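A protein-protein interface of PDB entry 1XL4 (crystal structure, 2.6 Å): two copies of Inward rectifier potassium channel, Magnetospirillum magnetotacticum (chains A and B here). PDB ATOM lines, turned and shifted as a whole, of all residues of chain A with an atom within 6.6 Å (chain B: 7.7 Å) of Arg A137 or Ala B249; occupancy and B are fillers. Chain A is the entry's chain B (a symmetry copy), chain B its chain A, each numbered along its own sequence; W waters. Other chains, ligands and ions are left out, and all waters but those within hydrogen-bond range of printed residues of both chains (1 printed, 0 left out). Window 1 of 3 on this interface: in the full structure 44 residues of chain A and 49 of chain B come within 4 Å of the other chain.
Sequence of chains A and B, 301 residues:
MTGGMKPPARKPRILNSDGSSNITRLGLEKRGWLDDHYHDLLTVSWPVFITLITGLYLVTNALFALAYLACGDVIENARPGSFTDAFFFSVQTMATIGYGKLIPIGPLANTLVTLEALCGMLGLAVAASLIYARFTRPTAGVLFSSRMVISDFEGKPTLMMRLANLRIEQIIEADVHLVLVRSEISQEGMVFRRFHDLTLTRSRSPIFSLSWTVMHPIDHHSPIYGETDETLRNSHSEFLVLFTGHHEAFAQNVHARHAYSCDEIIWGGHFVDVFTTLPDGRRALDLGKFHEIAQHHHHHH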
ATOM      1  N   ASP A  35      23.705 -28.099  -5.739  1.00  0.00           N
ATOM      2  CA  ASP A  35      25.025 -28.682  -5.540  1.00  0.00           C
ATOM      3  C   ASP A  35      24.987 -29.988  -4.761  1.00  0.00           C
ATOM      4  O   ASP A  35      25.902 -30.287  -3.992  1.00  0.00           O
ATOM      5  CB  ASP A  35      25.947 -27.691  -4.825  1.00  0.00           C
ATOM      6  CG  ASP A  35      26.449 -26.598  -5.744  1.00  0.00           C
ATOM      7  OD1 ASP A  35      27.120 -26.928  -6.744  1.00  0.00           O
ATOM      8  OD2 ASP A  35      26.175 -25.410  -5.468  1.00  0.00           O
ATOM      9  N   TYR A  38      24.891 -33.722  -7.631  1.00  0.00           N
ATOM     10  CA  TYR A  38      24.405 -33.477  -8.986  1.00  0.00           C
ATOM     11  C   TYR A  38      25.567 -33.557  -9.969  1.00  0.00           C
ATOM     12  O   TYR A  38      25.398 -33.958 -11.121  1.00  0.00           O
ATOM     13  CB  TYR A  38      23.736 -32.091  -9.031  1.00  0.00           C
ATOM     14  CG  TYR A  38      23.767 -31.367 -10.365  1.00  0.00           C
ATOM     15  CD1 TYR A  38      23.181 -31.918 -11.504  1.00  0.00           C
ATOM     16  CD2 TYR A  38      24.369 -30.112 -10.478  1.00  0.00           C
ATOM     17  CE1 TYR A  38      23.196 -31.236 -12.727  1.00  0.00           C
ATOM     18  CE2 TYR A  38      24.388 -29.423 -11.690  1.00  0.00           C
ATOM     19  CZ  TYR A  38      23.802 -29.990 -12.809  1.00  0.00           C
ATOM     20  OH  TYR A  38      23.830 -29.312 -14.008  1.00  0.00           O
ATOM     21  N   HIS A  39      26.750 -33.182  -9.499  1.00  0.00           N
ATOM     22  CA  HIS A  39      27.949 -33.224 -10.327  1.00  0.00           C
ATOM     23  C   HIS A  39      28.251 -34.686 -10.627  1.00  0.00           C
ATOM     24  O   HIS A  39      28.787 -35.017 -11.685  1.00  0.00           O
ATOM     25  CB  HIS A  39      29.122 -32.600  -9.576  1.00  0.00           C
ATOM     26  CG  HIS A  39      28.811 -31.261  -8.991  1.00  0.00           C
ATOM     27  ND1 HIS A  39      28.489 -30.169  -9.766  1.00  0.00           N
ATOM     28  CD2 HIS A  39      28.744 -30.845  -7.705  1.00  0.00           C
ATOM     29  CE1 HIS A  39      28.234 -29.136  -8.982  1.00  0.00           C
ATOM     30  NE2 HIS A  39      28.383 -29.520  -7.726  1.00  0.00           N
ATOM     31  N   LEU A  42      26.463 -35.939 -13.463  1.00  0.00           N
ATOM     32  CA  LEU A  42      27.002 -35.357 -14.687  1.00  0.00           C
ATOM     33  C   LEU A  42      28.264 -36.076 -15.155  1.00  0.00           C
ATOM     34  O   LEU A  42      28.523 -36.184 -16.354  1.00  0.00           O
ATOM     35  CB  LEU A  42      27.334 -33.880 -14.457  1.00  0.00           C
ATOM     36  CG  LEU A  42      26.198 -32.897 -14.169  1.00  0.00           C
ATOM     37  CD1 LEU A  42      26.748 -31.664 -13.473  1.00  0.00           C
ATOM     38  CD2 LEU A  42      25.506 -32.522 -15.470  1.00  0.00           C
ATOM     39  N   THR A  43      29.039 -36.574 -14.197  1.00  0.00           N
ATOM     40  CA  THR A  43      30.303 -37.242 -14.488  1.00  0.00           C
ATOM     41  C   THR A  43      30.237 -38.762 -14.601  1.00  0.00           C
ATOM     42  O   THR A  43      30.777 -39.350 -15.542  1.00  0.00           O
ATOM     43  CB  THR A  43      31.342 -36.900 -13.408  1.00  0.00           C
ATOM     44  OG1 THR A  43      31.040 -35.611 -12.853  1.00  0.00           O
ATOM     45  CG2 THR A  43      32.751 -36.883 -14.009  1.00  0.00           C
ATOM     46  N   TYR A 132      20.668 -34.320 -21.589  1.00  0.00           N
ATOM     47  CA  TYR A 132      21.168 -33.368 -22.568  1.00  0.00           C
ATOM     48  C   TYR A 132      22.432 -32.703 -22.037  1.00  0.00           C
ATOM     49  O   TYR A 132      23.322 -32.336 -22.809  1.00  0.00           O
ATOM     50  CB  TYR A 132      20.138 -32.282 -22.902  1.00  0.00           C
ATOM     51  CG  TYR A 132      20.666 -31.354 -23.980  1.00  0.00           C
ATOM     52  CD1 TYR A 132      20.793 -31.793 -25.301  1.00  0.00           C
ATOM     53  CD2 TYR A 132      21.164 -30.089 -23.659  1.00  0.00           C
ATOM     54  CE1 TYR A 132      21.414 -31.003 -26.273  1.00  0.00           C
ATOM     55  CE2 TYR A 132      21.786 -29.289 -24.621  1.00  0.00           C
ATOM     56  CZ  TYR A 132      21.914 -29.755 -25.923  1.00  0.00           C
ATOM     57  OH  TYR A 132      22.574 -28.995 -26.863  1.00  0.00           O
ATOM     58  N   ALA A 133      22.509 -32.542 -20.719  1.00  0.00           N
ATOM     59  CA  ALA A 133      23.671 -31.923 -20.106  1.00  0.00           C
ATOM     60  C   ALA A 133      24.866 -32.817 -20.341  1.00  0.00           C
ATOM     61  O   ALA A 133      25.852 -32.397 -20.937  1.00  0.00           O
ATOM     62  CB  ALA A 133      23.455 -31.733 -18.615  1.00  0.00           C
ATOM     63  N   ARG A 134      24.771 -34.055 -19.871  1.00  0.00           N
ATOM     64  CA  ARG A 134      25.847 -35.017 -20.025  1.00  0.00           C
ATOM     65  C   ARG A 134      26.298 -35.099 -21.476  1.00  0.00           C
ATOM     66  O   ARG A 134      27.457 -35.385 -21.759  1.00  0.00           O
ATOM     67  CB  ARG A 134      25.393 -36.383 -19.513  1.00  0.00           C
ATOM     68  CG  ARG A 134      25.288 -36.459 -17.985  1.00  0.00           C
ATOM     69  CD  ARG A 134      24.452 -37.657 -17.524  1.00  0.00           C
ATOM     70  NE  ARG A 134      24.971 -38.935 -18.010  1.00  0.00           N
ATOM     71  CZ  ARG A 134      26.027 -39.563 -17.500  1.00  0.00           C
ATOM     72  NH1 ARG A 134      26.691 -39.042 -16.474  1.00  0.00           N
ATOM     73  NH2 ARG A 134      26.424 -40.711 -18.027  1.00  0.00           N
ATOM     74  N   PHE A 135      25.376 -34.836 -22.396  1.00  0.00           N
ATOM     75  CA  PHE A 135      25.690 -34.861 -23.820  1.00  0.00           C
ATOM     76  C   PHE A 135      26.543 -33.647 -24.190  1.00  0.00           C
ATOM     77  O   PHE A 135      27.340 -33.697 -25.131  1.00  0.00           O
ATOM     78  CB  PHE A 135      24.415 -34.813 -24.671  1.00  0.00           C
ATOM     79  CG  PHE A 135      23.782 -36.155 -24.932  1.00  0.00           C
ATOM     80  CD1 PHE A 135      24.557 -37.288 -25.115  1.00  0.00           C
ATOM     81  CD2 PHE A 135      22.403 -36.262 -25.072  1.00  0.00           C
ATOM     82  CE1 PHE A 135      23.970 -38.512 -25.435  1.00  0.00           C
ATOM     83  CE2 PHE A 135      21.807 -37.478 -25.394  1.00  0.00           C
ATOM     84  CZ  PHE A 135      22.593 -38.604 -25.577  1.00  0.00           C
ATOM     85  N   THR A 136      26.373 -32.558 -23.445  1.00  0.00           N
ATOM     86  CA  THR A 136      27.096 -31.328 -23.732  1.00  0.00           C
ATOM     87  C   THR A 136      28.324 -31.007 -22.873  1.00  0.00           C
ATOM     88  O   THR A 136      28.715 -29.844 -22.751  1.00  0.00           O
ATOM     89  CB  THR A 136      26.131 -30.113 -23.714  1.00  0.00           C
ATOM     90  OG1 THR A 136      25.570 -29.950 -22.403  1.00  0.00           O
ATOM     91  CG2 THR A 136      25.014 -30.318 -24.731  1.00  0.00           C
ATOM     92  N   ARG A 137      28.928 -32.020 -22.265  1.00  0.00           N
ATOM     93  CA  ARG A 137      30.146 -31.797 -21.496  1.00  0.00           C
ATOM     94  C   ARG A 137      31.157 -32.845 -21.964  1.00  0.00           C
ATOM     95  O   ARG A 137      31.675 -33.635 -21.172  1.00  0.00           O
ATOM     96  CB  ARG A 137      29.896 -31.911 -19.988  1.00  0.00           C
ATOM     97  CG  ARG A 137      29.466 -33.273 -19.481  1.00  0.00           C
ATOM     98  CD  ARG A 137      29.936 -33.458 -18.041  1.00  0.00           C
ATOM     99  NE  ARG A 137      29.568 -32.327 -17.192  1.00  0.00           N
ATOM    100  CZ  ARG A 137      30.086 -32.094 -15.989  1.00  0.00           C
ATOM    101  NH1 ARG A 137      31.000 -32.915 -15.483  1.00  0.00           N
ATOM    102  NH2 ARG A 137      29.695 -31.036 -15.291  1.00  0.00           N
ATOM    103  N   PRO A 138      31.454 -32.853 -23.278  1.00  0.00           N
ATOM    104  CA  PRO A 138      32.388 -33.784 -23.917  1.00  0.00           C
ATOM    105  C   PRO A 138      33.845 -33.577 -23.538  1.00  0.00           C
ATOM    106  O   PRO A 138      34.244 -32.489 -23.118  1.00  0.00           O
ATOM    107  CB  PRO A 138      32.163 -33.535 -25.409  1.00  0.00           C
ATOM    108  CG  PRO A 138      30.817 -32.860 -25.473  1.00  0.00           C
ATOM    109  CD  PRO A 138      30.873 -31.960 -24.289  1.00  0.00           C
ATOM    110  N   THR A 139      34.628 -34.636 -23.710  1.00  0.00           N
ATOM    111  CA  THR A 139      36.054 -34.612 -23.414  1.00  0.00           C
ATOM    112  C   THR A 139      36.803 -34.063 -24.618  1.00  0.00           C
ATOM    113  O   THR A 139      36.394 -34.272 -25.757  1.00  0.00           O
ATOM    114  CB  THR A 139      36.579 -36.021 -23.120  1.00  0.00           C
ATOM    115  OG1 THR A 139      36.191 -36.901 -24.183  1.00  0.00           O
ATOM    116  CG2 THR A 139      36.017 -36.536 -21.802  1.00  0.00           C
ATOM    117  N   GLN A 252      31.026 -27.177 -29.531  1.00  0.00           N
ATOM    118  CA  GLN A 252      31.144 -26.470 -28.260  1.00  0.00           C
ATOM    119  C   GLN A 252      32.591 -26.605 -27.803  1.00  0.00           C
ATOM    120  O   GLN A 252      33.273 -27.565 -28.169  1.00  0.00           O
ATOM    121  CB  GLN A 252      30.209 -27.071 -27.210  1.00  0.00           C
ATOM    122  CG  GLN A 252      30.775 -28.293 -26.509  1.00  0.00           C
ATOM    123  CD  GLN A 252      30.037 -28.620 -25.220  1.00  0.00           C
ATOM    124  OE1 GLN A 252      30.619 -29.172 -24.278  1.00  0.00           O
ATOM    125  NE2 GLN A 252      28.745 -28.285 -25.174  1.00  0.00           N
ATOM    126  N   TYR B 132      16.113 -26.968 -17.164  1.00  0.00           N
ATOM    127  CA  TYR B 132      17.437 -27.058 -17.770  1.00  0.00           C
ATOM    128  C   TYR B 132      18.178 -25.732 -17.618  1.00  0.00           C
ATOM    129  O   TYR B 132      19.347 -25.703 -17.231  1.00  0.00           O
ATOM    130  CB  TYR B 132      17.349 -27.407 -19.255  1.00  0.00           C
ATOM    131  CG  TYR B 132      18.714 -27.567 -19.878  1.00  0.00           C
ATOM    132  CD1 TYR B 132      19.457 -28.733 -19.689  1.00  0.00           C
ATOM    133  CD2 TYR B 132      19.287 -26.538 -20.621  1.00  0.00           C
ATOM    134  CE1 TYR B 132      20.738 -28.868 -20.228  1.00  0.00           C
ATOM    135  CE2 TYR B 132      20.565 -26.660 -21.161  1.00  0.00           C
ATOM    136  CZ  TYR B 132      21.281 -27.829 -20.961  1.00  0.00           C
ATOM    137  OH  TYR B 132      22.537 -27.954 -21.515  1.00  0.00           O
ATOM    138  N   PRO B 138      25.032 -21.805 -13.063  1.00  0.00           N
ATOM    139  CA  PRO B 138      25.735 -22.124 -11.819  1.00  0.00           C
ATOM    140  C   PRO B 138      26.377 -20.887 -11.228  1.00  0.00           C
ATOM    141  O   PRO B 138      26.725 -19.950 -11.947  1.00  0.00           O
ATOM    142  CB  PRO B 138      26.799 -23.129 -12.260  1.00  0.00           C
ATOM    143  CG  PRO B 138      26.266 -23.679 -13.540  1.00  0.00           C
ATOM    144  CD  PRO B 138      25.685 -22.467 -14.199  1.00  0.00           C
ATOM    145  N   THR B 139      26.535 -20.886  -9.913  1.00  0.00           N
ATOM    146  CA  THR B 139      27.173 -19.768  -9.253  1.00  0.00           C
ATOM    147  C   THR B 139      28.667 -20.057  -9.324  1.00  0.00           C
ATOM    148  O   THR B 139      29.073 -21.217  -9.434  1.00  0.00           O
ATOM    149  CB  THR B 139      26.710 -19.656  -7.792  1.00  0.00           C
ATOM    150  OG1 THR B 139      26.980 -20.882  -7.101  1.00  0.00           O
ATOM    151  CG2 THR B 139      25.218 -19.363  -7.739  1.00  0.00           C
ATOM    152  N   ARG B 167      34.471 -24.243  -3.606  1.00  0.00           N
ATOM    153  CA  ARG B 167      34.133 -25.612  -3.967  1.00  0.00           C
ATOM    154  C   ARG B 167      35.406 -26.432  -4.087  1.00  0.00           C
ATOM    155  O   ARG B 167      36.498 -25.883  -4.179  1.00  0.00           O
ATOM    156  CB  ARG B 167      33.384 -25.655  -5.295  1.00  0.00           C
ATOM    157  CG  ARG B 167      32.001 -25.020  -5.295  1.00  0.00           C
ATOM    158  CD  ARG B 167      31.420 -25.130  -6.691  1.00  0.00           C
ATOM    159  NE  ARG B 167      30.637 -23.964  -7.092  1.00  0.00           N
ATOM    160  CZ  ARG B 167      29.341 -23.817  -6.852  1.00  0.00           C
ATOM    161  NH1 ARG B 167      28.679 -24.766  -6.208  1.00  0.00           N
ATOM    162  NH2 ARG B 167      28.704 -22.732  -7.267  1.00  0.00           N
ATOM    163  N   ILE B 168      35.260 -27.753  -4.085  1.00  0.00           N
ATOM    164  CA  ILE B 168      36.405 -28.656  -4.194  1.00  0.00           C
ATOM    165  C   ILE B 168      36.862 -28.703  -5.642  1.00  0.00           C
ATOM    166  O   ILE B 168      38.050 -28.837  -5.925  1.00  0.00           O
ATOM    167  CB  ILE B 168      36.037 -30.088  -3.749  1.00  0.00           C
ATOM    168  CG1 ILE B 168      35.441 -30.054  -2.338  1.00  0.00           C
ATOM    169  CG2 ILE B 168      37.268 -30.976  -3.775  1.00  0.00           C
ATOM    170  CD1 ILE B 168      34.825 -31.374  -1.887  1.00  0.00           C
ATOM    171  N   GLU B 169      35.910 -28.607  -6.562  1.00  0.00           N
ATOM    172  CA  GLU B 169      36.250 -28.624  -7.975  1.00  0.00           C
ATOM    173  C   GLU B 169      36.940 -27.308  -8.317  1.00  0.00           C
ATOM    174  O   GLU B 169      36.605 -26.251  -7.779  1.00  0.00           O
ATOM    175  CB  GLU B 169      35.001 -28.808  -8.837  1.00  0.00           C
ATOM    176  CG  GLU B 169      34.220 -30.068  -8.518  1.00  0.00           C
ATOM    177  CD  GLU B 169      33.178 -29.847  -7.438  1.00  0.00           C
ATOM    178  OE1 GLU B 169      33.388 -28.962  -6.573  1.00  0.00           O
ATOM    179  OE2 GLU B 169      32.153 -30.565  -7.449  1.00  0.00           O
ATOM    180  N   GLN B 170      37.904 -27.384  -9.220  1.00  0.00           N
ATOM    181  CA  GLN B 170      38.672 -26.221  -9.617  1.00  0.00           C
ATOM    182  C   GLN B 170      38.085 -25.470 -10.794  1.00  0.00           C
ATOM    183  O   GLN B 170      37.350 -26.023 -11.604  1.00  0.00           O
ATOM    184  CB  GLN B 170      40.096 -26.656  -9.950  1.00  0.00           C
ATOM    185  CG  GLN B 170      40.730 -27.489  -8.848  1.00  0.00           C
ATOM    186  CD  GLN B 170      41.969 -28.210  -9.314  1.00  0.00           C
ATOM    187  OE1 GLN B 170      41.926 -28.966 -10.284  1.00  0.00           O
ATOM    188  NE2 GLN B 170      43.085 -27.983  -8.630  1.00  0.00           N
ATOM    189  N   ILE B 171      38.408 -24.187 -10.858  1.00  0.00           N
ATOM    190  CA  ILE B 171      37.965 -23.328 -11.934  1.00  0.00           C
ATOM    191  C   ILE B 171      39.246 -23.114 -12.727  1.00  0.00           C
ATOM    192  O   ILE B 171      40.296 -22.816 -12.150  1.00  0.00           O
ATOM    193  CB  ILE B 171      37.435 -21.976 -11.383  1.00  0.00           C
ATOM    194  CG1 ILE B 171      36.284 -22.236 -10.401  1.00  0.00           C
ATOM    195  CG2 ILE B 171      36.978 -21.082 -12.523  1.00  0.00           C
ATOM    196  CD1 ILE B 171      35.714 -20.990  -9.745  1.00  0.00           C
ATOM    197  N   HIS B 246      36.341 -21.111 -16.150  1.00  0.00           N
ATOM    198  CA  HIS B 246      35.606 -22.273 -16.595  1.00  0.00           C
ATOM    199  C   HIS B 246      35.547 -23.178 -15.390  1.00  0.00           C
ATOM    200  O   HIS B 246      36.574 -23.651 -14.905  1.00  0.00           O
ATOM    201  CB  HIS B 246      36.316 -22.990 -17.752  1.00  0.00           C
ATOM    202  CG  HIS B 246      35.538 -24.149 -18.291  1.00  0.00           C
ATOM    203  ND1 HIS B 246      34.352 -23.988 -18.977  1.00  0.00           N
ATOM    204  CD2 HIS B 246      35.714 -25.486 -18.153  1.00  0.00           C
ATOM    205  CE1 HIS B 246      33.827 -25.175 -19.230  1.00  0.00           C
ATOM    206  NE2 HIS B 246      34.632 -26.101 -18.741  1.00  0.00           N
ATOM    207  N   HIS B 247      34.341 -23.402 -14.892  1.00  0.00           N
ATOM    208  CA  HIS B 247      34.167 -24.260 -13.742  1.00  0.00           C
ATOM    209  C   HIS B 247      34.025 -25.706 -14.208  1.00  0.00           C
ATOM    210  O   HIS B 247      33.060 -26.059 -14.883  1.00  0.00           O
ATOM    211  CB  HIS B 247      32.931 -23.835 -12.949  1.00  0.00           C
ATOM    212  CG  HIS B 247      33.081 -24.032 -11.474  1.00  0.00           C
ATOM    213  ND1 HIS B 247      33.369 -25.258 -10.914  1.00  0.00           N
ATOM    214  CD2 HIS B 247      33.037 -23.149 -10.448  1.00  0.00           C
ATOM    215  CE1 HIS B 247      33.497 -25.121  -9.607  1.00  0.00           C
ATOM    216  NE2 HIS B 247      33.299 -23.852  -9.299  1.00  0.00           N
ATOM    217  N   GLU B 248      34.997 -26.540 -13.853  1.00  0.00           N
ATOM    218  CA  GLU B 248      34.961 -27.942 -14.244  1.00  0.00           C
ATOM    219  C   GLU B 248      33.773 -28.664 -13.623  1.00  0.00           C
ATOM    220  O   GLU B 248      33.237 -29.606 -14.206  1.00  0.00           O
ATOM    221  CB  GLU B 248      36.259 -28.642 -13.838  1.00  0.00           C
ATOM    222  CG  GLU B 248      37.496 -28.037 -14.467  1.00  0.00           C
ATOM    223  CD  GLU B 248      38.665 -28.994 -14.486  1.00  0.00           C
ATOM    224  OE1 GLU B 248      38.953 -29.598 -13.431  1.00  0.00           O
ATOM    225  OE2 GLU B 248      39.298 -29.136 -15.554  1.00  0.00           O
ATOM    226  N   ALA B 249      33.367 -28.218 -12.436  1.00  0.00           N
ATOM    227  CA  ALA B 249      32.240 -28.819 -11.736  1.00  0.00           C
ATOM    228  C   ALA B 249      31.004 -28.893 -12.624  1.00  0.00           C
ATOM    229  O   ALA B 249      30.333 -29.920 -12.669  1.00  0.00           O
ATOM    230  CB  ALA B 249      31.925 -28.026 -10.482  1.00  0.00           C
ATOM    231  N   PHE B 250      30.718 -27.807 -13.338  1.00  0.00           N
ATOM    232  CA  PHE B 250      29.545 -27.734 -14.209  1.00  0.00           C
ATOM    233  C   PHE B 250      29.908 -27.774 -15.686  1.00  0.00           C
ATOM    234  O   PHE B 250      29.036 -27.738 -16.552  1.00  0.00           O
ATOM    235  CB  PHE B 250      28.762 -26.448 -13.936  1.00  0.00           C
ATOM    236  CG  PHE B 250      28.707 -26.067 -12.489  1.00  0.00           C
ATOM    237  CD1 PHE B 250      29.671 -25.224 -11.943  1.00  0.00           C
ATOM    238  CD2 PHE B 250      27.695 -26.556 -11.665  1.00  0.00           C
ATOM    239  CE1 PHE B 250      29.631 -24.871 -10.594  1.00  0.00           C
ATOM    240  CE2 PHE B 250      27.647 -26.211 -10.316  1.00  0.00           C
ATOM    241  CZ  PHE B 250      28.616 -25.366  -9.779  1.00  0.00           C
ATOM    242  N   ALA B 251      31.201 -27.839 -15.963  1.00  0.00           N
ATOM    243  CA  ALA B 251      31.691 -27.873 -17.331  1.00  0.00           C
ATOM    244  C   ALA B 251      31.237 -26.650 -18.124  1.00  0.00           C
ATOM    245  O   ALA B 251      31.080 -26.712 -19.341  1.00  0.00           O
ATOM    246  CB  ALA B 251      31.236 -29.156 -18.019  1.00  0.00           C
ATOM    247  N   GLN B 252      31.009 -25.541 -17.432  1.00  0.00           N
ATOM    248  CA  GLN B 252      30.631 -24.299 -18.100  1.00  0.00           C
ATOM    249  C   GLN B 252      31.234 -23.090 -17.399  1.00  0.00           C
ATOM    250  O   GLN B 252      31.663 -23.185 -16.249  1.00  0.00           O
ATOM    251  CB  GLN B 252      29.109 -24.160 -18.216  1.00  0.00           C
ATOM    252  CG  GLN B 252      28.303 -24.433 -16.975  1.00  0.00           C
ATOM    253  CD  GLN B 252      26.852 -24.693 -17.333  1.00  0.00           C
ATOM    254  OE1 GLN B 252      26.552 -25.567 -18.157  1.00  0.00           O
ATOM    255  NE2 GLN B 252      25.942 -23.937 -16.726  1.00  0.00           N
HETATM  256  O   HOH W   1      27.661 -30.194 -17.858  1.00  0.00           O
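OG1 of Thr B139 sits at hydrogen-bond distance from NH2 of Arg B167, 2.5 Å away. A ring nitrogen (NE2) of His B247 lies close to the guanidinium group (NE) of Arg B167. O of Gln B170 lies within hydrogen-bond range of N of Glu B248, at 3.3 Å. The side-chain carboxylate (OD1) of Asp A35 lies within hydrogen-bond range of a ring nitrogen (NE2) of His A39 (3.0 Å). The backbone carbonyl oxygen (O) of Tyr A132 sits close to the side-chain hydroxyl (OG1) of Thr A136 (3.3 Å). The backbone carbonyl oxygen (O) of Thr A136 sits close to the side-chain amide oxygen (OE1) of Gln A252, 2.5 Å away.
OD2 of Asp A35 lies within salt-bridge range of NH1 of Arg B167. The backbone carbonyl oxygen (O) of Ala B249 is in hydrogen-bond range of a ring nitrogen (ND1) of His A39 (3.4 Å). O of Ala B249 is in hydrogen-bond range of NH2 of Arg A137.
Of the 15 printed residues of chain B, 7 touch a printed residue of chain A. Hydrophobic or aromatic side chains of chain B that line the printed part of chain A: Tyr B132, Phe B250 and Ala B251. Among the printed residues, Asp or Glu carboxylates within 4 Å of a Lys or Arg side-chain nitrogen of the other chain: Asp A35 with Arg B167.
Tyr A132 touches its own counterpart, Tyr B132.
Printed residues of chain B within 4 Å of Asp A35: Arg B167 and Phe B250. Gln A252 touches none of the printed residues of chain B. Of the printed residues of chain A, Tyr B132 touches Tyr A132 and Thr A136. Thr B139 touches none of the printed residues of chain A. Of the printed residues of chain A, Ala B249 touches His A39 and Arg A137. Printed residues of chain A within 4 Å of Ala B251: Arg A137 (3.6 Å). The nearest printed residue of chain B that does not touch Arg A137 is His B247 (6.0 Å). The nearest residue of chain A that does not touch Ala B249 is Leu A42 (4.1 Å). The nearest printed residue of chain B that does not touch Asp A35 is Thr B139 (4.9 Å).
Water W1 bridges the guanidinium group of Arg A137 (2.9 Å) and the backbone carbonyl oxygen of Phe B250 (3.1 Å).
CE2 of Phe B250 touches OD1 of Asp A35 (3.7 Å). Glu B169 touches His A39 (OE2 to CD2, 3.4 Å). His A39 touches Phe B250 (CE1 to CE2, 3.3 Å). Tyr B132 touches Tyr A132 (OH to CD2, 3.3 Å). Thr A136 touches Tyr B132 (OG1 to OH, 3.7 Å). Arg A137 touches Glu B248. Arg A137 touches Phe B250. Arg A137 touches Ala B251.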
